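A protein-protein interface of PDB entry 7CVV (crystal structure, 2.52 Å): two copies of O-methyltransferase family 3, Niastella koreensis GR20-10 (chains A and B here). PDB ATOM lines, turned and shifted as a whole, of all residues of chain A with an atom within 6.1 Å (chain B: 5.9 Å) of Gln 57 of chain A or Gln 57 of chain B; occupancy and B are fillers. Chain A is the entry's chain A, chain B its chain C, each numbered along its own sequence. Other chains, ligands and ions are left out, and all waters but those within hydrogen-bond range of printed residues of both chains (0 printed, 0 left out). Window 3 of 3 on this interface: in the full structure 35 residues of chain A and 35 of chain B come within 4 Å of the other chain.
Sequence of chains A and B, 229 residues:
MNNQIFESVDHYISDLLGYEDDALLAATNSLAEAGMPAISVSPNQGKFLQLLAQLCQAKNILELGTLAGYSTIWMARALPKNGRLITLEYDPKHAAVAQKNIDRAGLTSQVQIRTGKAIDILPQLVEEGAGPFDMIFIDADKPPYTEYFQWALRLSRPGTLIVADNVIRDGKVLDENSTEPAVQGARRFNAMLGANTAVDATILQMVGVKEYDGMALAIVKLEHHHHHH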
ATOM      1  N   LEU A  52       0.464  -1.020  25.540  1.00  0.00           N
ATOM      2  CA  LEU A  52      -0.929  -0.601  25.276  1.00  0.00           C
ATOM      3  C   LEU A  52      -1.388  -1.220  23.952  1.00  0.00           C
ATOM      4  O   LEU A  52      -2.553  -1.649  23.858  1.00  0.00           O
ATOM      5  CB  LEU A  52      -0.972   0.926  25.238  1.00  0.00           C
ATOM      6  CG  LEU A  52      -0.719   1.610  26.582  1.00  0.00           C
ATOM      7  CD1 LEU A  52      -0.489   3.090  26.375  1.00  0.00           C
ATOM      8  CD2 LEU A  52      -1.863   1.380  27.559  1.00  0.00           C
ATOM      9  N   ALA A  53      -0.492  -1.259  22.964  1.00  0.00           N
ATOM     10  CA  ALA A  53      -0.777  -1.789  21.619  1.00  0.00           C
ATOM     11  C   ALA A  53      -1.108  -3.272  21.775  1.00  0.00           C
ATOM     12  O   ALA A  53      -2.176  -3.684  21.309  1.00  0.00           O
ATOM     13  CB  ALA A  53       0.395  -1.543  20.704  1.00  0.00           C
ATOM     14  N   GLN A  54      -0.252  -4.007  22.486  1.00  0.00           N
ATOM     15  CA  GLN A  54      -0.444  -5.438  22.867  1.00  0.00           C
ATOM     16  C   GLN A  54      -1.748  -5.614  23.659  1.00  0.00           C
ATOM     17  O   GLN A  54      -2.426  -6.604  23.397  1.00  0.00           O
ATOM     18  CB  GLN A  54       0.751  -5.963  23.660  1.00  0.00           C
ATOM     19  CG  GLN A  54       2.070  -5.963  22.904  1.00  0.00           C
ATOM     20  CD  GLN A  54       3.171  -6.494  23.786  1.00  0.00           C
ATOM     21  OE1 GLN A  54       3.973  -5.748  24.336  1.00  0.00           O
ATOM     22  NE2 GLN A  54       3.186  -7.799  23.989  1.00  0.00           N
ATOM     23  N   LEU A  55      -2.119  -4.678  24.541  1.00  0.00           N
ATOM     24  CA  LEU A  55      -3.393  -4.735  25.319  1.00  0.00           C
ATOM     25  C   LEU A  55      -4.628  -4.543  24.426  1.00  0.00           C
ATOM     26  O   LEU A  55      -5.663  -5.095  24.801  1.00  0.00           O
ATOM     27  CB  LEU A  55      -3.385  -3.698  26.444  1.00  0.00           C
ATOM     28  CG  LEU A  55      -2.712  -4.159  27.732  1.00  0.00           C
ATOM     29  CD1 LEU A  55      -2.573  -3.010  28.718  1.00  0.00           C
ATOM     30  CD2 LEU A  55      -3.462  -5.331  28.362  1.00  0.00           C
ATOM     31  N   CYS A  56      -4.555  -3.774  23.331  1.00  0.00           N
ATOM     32  CA  CYS A  56      -5.636  -3.645  22.302  1.00  0.00           C
ATOM     33  C   CYS A  56      -5.595  -4.791  21.293  1.00  0.00           C
ATOM     34  O   CYS A  56      -6.393  -4.727  20.330  1.00  0.00           O
ATOM     35  CB  CYS A  56      -5.480  -2.413  21.428  1.00  0.00           C
ATOM     36  SG  CYS A  56      -5.240  -0.919  22.401  1.00  0.00           S
ATOM     37  N   GLN A  57      -4.646  -5.725  21.448  1.00  0.00           N
ATOM     38  CA  GLN A  57      -4.441  -6.851  20.509  1.00  0.00           C
ATOM     39  C   GLN A  57      -4.349  -6.276  19.096  1.00  0.00           C
ATOM     40  O   GLN A  57      -5.019  -6.784  18.199  1.00  0.00           O
ATOM     41  CB  GLN A  57      -5.575  -7.861  20.681  1.00  0.00           C
ATOM     42  CG  GLN A  57      -5.438  -8.644  21.970  1.00  0.00           C
ATOM     43  CD  GLN A  57      -6.598  -9.573  22.206  1.00  0.00           C
ATOM     44  OE1 GLN A  57      -6.411 -10.761  22.456  1.00  0.00           O
ATOM     45  NE2 GLN A  57      -7.802  -9.033  22.141  1.00  0.00           N
ATOM     46  N   ALA A  58      -3.531  -5.243  18.941  1.00  0.00           N
ATOM     47  CA  ALA A  58      -3.389  -4.403  17.735  1.00  0.00           C
ATOM     48  C   ALA A  58      -2.937  -5.228  16.525  1.00  0.00           C
ATOM     49  O   ALA A  58      -1.831  -5.824  16.592  1.00  0.00           O
ATOM     50  CB  ALA A  58      -2.375  -3.341  18.050  1.00  0.00           C
ATOM     51  N   LYS A  59      -3.749  -5.241  15.460  1.00  0.00           N
ATOM     52  CA  LYS A  59      -3.323  -5.652  14.090  1.00  0.00           C
ATOM     53  C   LYS A  59      -3.217  -4.399  13.208  1.00  0.00           C
ATOM     54  O   LYS A  59      -2.518  -4.451  12.173  1.00  0.00           O
ATOM     55  CB  LYS A  59      -4.299  -6.662  13.462  1.00  0.00           C
ATOM     56  CG  LYS A  59      -4.797  -7.776  14.375  1.00  0.00           C
ATOM     57  CD  LYS A  59      -3.700  -8.689  14.908  1.00  0.00           C
ATOM     58  CE  LYS A  59      -3.742  -8.887  16.415  1.00  0.00           C
ATOM     59  NZ  LYS A  59      -3.384 -10.270  16.819  1.00  0.00           N
ATOM     60  N   ASN A  60      -3.882  -3.314  13.612  1.00  0.00           N
ATOM     61  CA  ASN A  60      -4.064  -2.072  12.819  1.00  0.00           C
ATOM     62  C   ASN A  60      -3.877  -0.840  13.696  1.00  0.00           C
ATOM     63  O   ASN A  60      -4.769  -0.614  14.511  1.00  0.00           O
ATOM     64  CB  ASN A  60      -5.476  -1.983  12.258  1.00  0.00           C
ATOM     65  CG  ASN A  60      -5.513  -2.310  10.791  1.00  0.00           C
ATOM     66  OD1 ASN A  60      -5.259  -1.437   9.962  1.00  0.00           O
ATOM     67  ND2 ASN A  60      -5.800  -3.564  10.485  1.00  0.00           N
ATOM     68  N   ASP A 134      -7.152  -0.500  15.905  1.00  0.00           N
ATOM     69  CA  ASP A 134      -7.135  -1.076  17.269  1.00  0.00           C
ATOM     70  C   ASP A 134      -6.669  -0.004  18.248  1.00  0.00           C
ATOM     71  O   ASP A 134      -7.246   0.102  19.353  1.00  0.00           O
ATOM     72  CB  ASP A 134      -6.233  -2.302  17.272  1.00  0.00           C
ATOM     73  CG  ASP A 134      -6.820  -3.381  16.387  1.00  0.00           C
ATOM     74  OD1 ASP A 134      -8.014  -3.647  16.574  1.00  0.00           O
ATOM     75  OD2 ASP A 134      -6.087  -3.902  15.504  1.00  0.00           O
ATOM     76  N   ARG A 157     -13.328   1.257  16.524  1.00  0.00           N
ATOM     77  CA  ARG A 157     -14.319   0.195  16.819  1.00  0.00           C
ATOM     78  C   ARG A 157     -14.553   0.234  18.318  1.00  0.00           C
ATOM     79  O   ARG A 157     -13.761   0.829  19.044  1.00  0.00           O
ATOM     80  CB  ARG A 157     -13.780  -1.164  16.375  1.00  0.00           C
ATOM     81  CG  ARG A 157     -12.352  -1.436  16.835  1.00  0.00           C
ATOM     82  CD  ARG A 157     -12.237  -2.513  17.886  1.00  0.00           C
ATOM     83  NE  ARG A 157     -10.872  -3.010  18.101  1.00  0.00           N
ATOM     84  CZ  ARG A 157     -10.386  -3.349  19.298  1.00  0.00           C
ATOM     85  NH1 ARG A 157     -11.137  -3.234  20.381  1.00  0.00           N
ATOM     86  NH2 ARG A 157      -9.149  -3.786  19.431  1.00  0.00           N
ATOM     87  N   LEU B  52      -7.885   0.440  32.225  1.00  0.00           N
ATOM     88  CA  LEU B  52      -7.042  -0.764  32.009  1.00  0.00           C
ATOM     89  C   LEU B  52      -7.916  -2.012  32.064  1.00  0.00           C
ATOM     90  O   LEU B  52      -7.739  -2.899  31.216  1.00  0.00           O
ATOM     91  CB  LEU B  52      -5.949  -0.841  33.073  1.00  0.00           C
ATOM     92  CG  LEU B  52      -4.841   0.192  32.937  1.00  0.00           C
ATOM     93  CD1 LEU B  52      -3.930   0.132  34.150  1.00  0.00           C
ATOM     94  CD2 LEU B  52      -4.054   0.005  31.644  1.00  0.00           C
ATOM     95  N   ALA B  53      -8.850  -2.071  33.009  1.00  0.00           N
ATOM     96  CA  ALA B  53      -9.746  -3.235  33.134  1.00  0.00           C
ATOM     97  C   ALA B  53     -10.568  -3.383  31.846  1.00  0.00           C
ATOM     98  O   ALA B  53     -10.687  -4.521  31.373  1.00  0.00           O
ATOM     99  CB  ALA B  53     -10.582  -3.132  34.383  1.00  0.00           C
ATOM    100  N   GLN B  54     -11.044  -2.290  31.239  1.00  0.00           N
ATOM    101  CA  GLN B  54     -11.893  -2.348  30.008  1.00  0.00           C
ATOM    102  C   GLN B  54     -11.063  -2.735  28.777  1.00  0.00           C
ATOM    103  O   GLN B  54     -11.565  -3.535  27.958  1.00  0.00           O
ATOM    104  CB  GLN B  54     -12.593  -1.020  29.756  1.00  0.00           C
ATOM    105  CG  GLN B  54     -13.455  -0.570  30.919  1.00  0.00           C
ATOM    106  CD  GLN B  54     -13.856   0.863  30.692  1.00  0.00           C
ATOM    107  OE1 GLN B  54     -13.402   1.776  31.376  1.00  0.00           O
ATOM    108  NE2 GLN B  54     -14.675   1.070  29.672  1.00  0.00           N
ATOM    109  N   LEU B  55      -9.848  -2.198  28.646  1.00  0.00           N
ATOM    110  CA  LEU B  55      -8.825  -2.661  27.666  1.00  0.00           C
ATOM    111  C   LEU B  55      -8.627  -4.179  27.744  1.00  0.00           C
ATOM    112  O   LEU B  55      -8.524  -4.787  26.672  1.00  0.00           O
ATOM    113  CB  LEU B  55      -7.497  -1.969  27.957  1.00  0.00           C
ATOM    114  CG  LEU B  55      -7.238  -0.689  27.177  1.00  0.00           C
ATOM    115  CD1 LEU B  55      -5.813  -0.230  27.409  1.00  0.00           C
ATOM    116  CD2 LEU B  55      -7.497  -0.883  25.693  1.00  0.00           C
ATOM    117  N   CYS B  56      -8.548  -4.755  28.952  1.00  0.00           N
ATOM    118  CA  CYS B  56      -8.397  -6.219  29.201  1.00  0.00           C
ATOM    119  C   CYS B  56      -9.726  -6.966  29.016  1.00  0.00           C
ATOM    120  O   CYS B  56      -9.736  -8.212  29.112  1.00  0.00           O
ATOM    121  CB  CYS B  56      -7.907  -6.494  30.616  1.00  0.00           C
ATOM    122  SG  CYS B  56      -6.321  -5.714  30.995  1.00  0.00           S
ATOM    123  N   GLN B  57     -10.818  -6.235  28.786  1.00  0.00           N
ATOM    124  CA  GLN B  57     -12.178  -6.792  28.538  1.00  0.00           C
ATOM    125  C   GLN B  57     -12.569  -7.620  29.765  1.00  0.00           C
ATOM    126  O   GLN B  57     -13.218  -8.672  29.618  1.00  0.00           O
ATOM    127  CB  GLN B  57     -12.198  -7.603  27.238  1.00  0.00           C
ATOM    128  CG  GLN B  57     -11.759  -6.817  26.015  1.00  0.00           C
ATOM    129  CD  GLN B  57     -11.916  -7.632  24.758  1.00  0.00           C
ATOM    130  OE1 GLN B  57     -12.897  -7.495  24.043  1.00  0.00           O
ATOM    131  NE2 GLN B  57     -10.959  -8.494  24.473  1.00  0.00           N
ATOM    132  N   ALA B  58     -12.182  -7.116  30.933  1.00  0.00           N
ATOM    133  CA  ALA B  58     -12.239  -7.818  32.227  1.00  0.00           C
ATOM    134  C   ALA B  58     -13.670  -8.317  32.507  1.00  0.00           C
ATOM    135  O   ALA B  58     -14.623  -7.521  32.375  1.00  0.00           O
ATOM    136  CB  ALA B  58     -11.692  -6.906  33.302  1.00  0.00           C
ATOM    137  N   LYS B  59     -13.796  -9.618  32.815  1.00  0.00           N
ATOM    138  CA  LYS B  59     -14.987 -10.270  33.432  1.00  0.00           C
ATOM    139  C   LYS B  59     -14.595 -10.835  34.807  1.00  0.00           C
ATOM    140  O   LYS B  59     -15.494 -10.926  35.666  1.00  0.00           O
ATOM    141  CB  LYS B  59     -15.544 -11.350  32.499  1.00  0.00           C
ATOM    142  CG  LYS B  59     -15.731 -10.917  31.048  1.00  0.00           C
ATOM    143  CD  LYS B  59     -17.148 -11.002  30.532  1.00  0.00           C
ATOM    144  CE  LYS B  59     -17.273 -10.630  29.063  1.00  0.00           C
ATOM    145  NZ  LYS B  59     -18.523 -11.148  28.446  1.00  0.00           N
ATOM    146  N   ASP B 134      -8.405 -11.638  34.072  1.00  0.00           N
ATOM    147  CA  ASP B 134      -8.234 -10.645  32.973  1.00  0.00           C
ATOM    148  C   ASP B 134      -7.217  -9.582  33.427  1.00  0.00           C
ATOM    149  O   ASP B 134      -6.375  -9.139  32.618  1.00  0.00           O
ATOM    150  CB  ASP B 134      -9.606 -10.055  32.610  1.00  0.00           C
ATOM    151  CG  ASP B 134     -10.585 -11.104  32.104  1.00  0.00           C
ATOM    152  OD1 ASP B 134     -10.184 -11.853  31.194  1.00  0.00           O
ATOM    153  OD2 ASP B 134     -11.715 -11.201  32.648  1.00  0.00           O
ATOM    154  N   ARG B 157      -3.888 -15.766  32.064  1.00  0.00           N
ATOM    155  CA  ARG B 157      -3.973 -16.274  30.674  1.00  0.00           C
ATOM    156  C   ARG B 157      -3.092 -15.363  29.828  1.00  0.00           C
ATOM    157  O   ARG B 157      -2.691 -14.294  30.298  1.00  0.00           O
ATOM    158  CB  ARG B 157      -5.422 -16.217  30.174  1.00  0.00           C
ATOM    159  CG  ARG B 157      -6.077 -14.859  30.374  1.00  0.00           C
ATOM    160  CD  ARG B 157      -6.764 -14.346  29.130  1.00  0.00           C
ATOM    161  NE  ARG B 157      -7.556 -13.145  29.392  1.00  0.00           N
ATOM    162  CZ  ARG B 157      -7.326 -11.950  28.864  1.00  0.00           C
ATOM    163  NH1 ARG B 157      -6.316 -11.763  28.026  1.00  0.00           N
ATOM    164  NH2 ARG B 157      -8.110 -10.937  29.189  1.00  0.00           N
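The backbone carbonyl oxygen (O) of Leu 55 of chain B sits close to the backbone carbonyl oxygen (O) of Leu 55 of chain A, 3.4 Å away.
O of Leu 52 of chain A lies within hydrogen-bond range of SG of Cys 56 of chain A, at 3.1 Å.
SG of Cys 56 of chain A sits close to O of Asp 134 of chain A (3.8 Å).
O of Cys 56 of chain A is in hydrogen-bond range of NH2 of Arg 157 of chain A (3.0 Å).
O of Leu 52 of chain B lies within hydrogen-bond range of SG of Cys 56 of chain B (3.2 Å).
The side-chain sulfur of Cys 56 of chain B sits close to the backbone carbonyl oxygen of Asp 134 of chain B, 3.8 Å away.
O of Cys 56 of chain B sits at hydrogen-bond distance from NH2 of Arg 157 of chain B, at 3.2 Å.
Among the printed residues, merely in contact across the chains: Leu 55 of chain A with Cys 56 of chain B (3.9 Å), Cys 56 of chain A with Leu 55 of chain B (3.99 Å) and Gln 57 of chain A with Gln 57 of chain B (3.96 Å).
Gln 57 of chain A touches just one residue of chain B: Gln 57 (3.96 Å).
Lys 59 of chain A touches none of the printed residues of chain B.
Asp 134 of chain A touches none of the printed residues of chain B.
Of the printed residues of chain A, Leu 55 of chain B touches Leu 55 and Cys 56.
Printed residues of chain A within 4 Å of Cys 56 of chain B: Leu 55 (3.9 Å).
Of chain A, only Gln 57 (3.96 Å) comes within 4 Å of Gln 57 of chain B.
The nearest residue of chain A that does not touch Gln 57 of chain B is Arg 157 of chain A (5.9 Å).
Printed residues of chain A that touch a printed residue of chain B: Leu 55, Cys 56 and Gln 57.
Hydrophobic or aromatic side chains of chain A within 4 Å of the printed part of chain B: Leu 55.
Hydrophobic or aromatic side chains of chain B within 4 Å of the printed part of chain A: Leu 55.
Along chain B the printed residues that touch a printed residue of chain A span positions 55 to 57.
Among the printed residues, no Asp or Glu carboxylate lies within 4 Å of a Lys or Arg side-chain nitrogen of the other chain.
Leu 55 of chain A touches its own counterpart, Leu 55 of chain B.
Leu 55 of chain A touches Cys 56 of chain B, and with the chains exchanged Cys 56 of chain A touches Leu 55 of chain B.
Gln 57 of chain B touches its own counterpart, Gln 57 of chain A.
10 positions are printed for both chains.
Of the 4 pairs that touch across the chains among the printed residues, 4 have their exchanged pair printed and touching as well.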
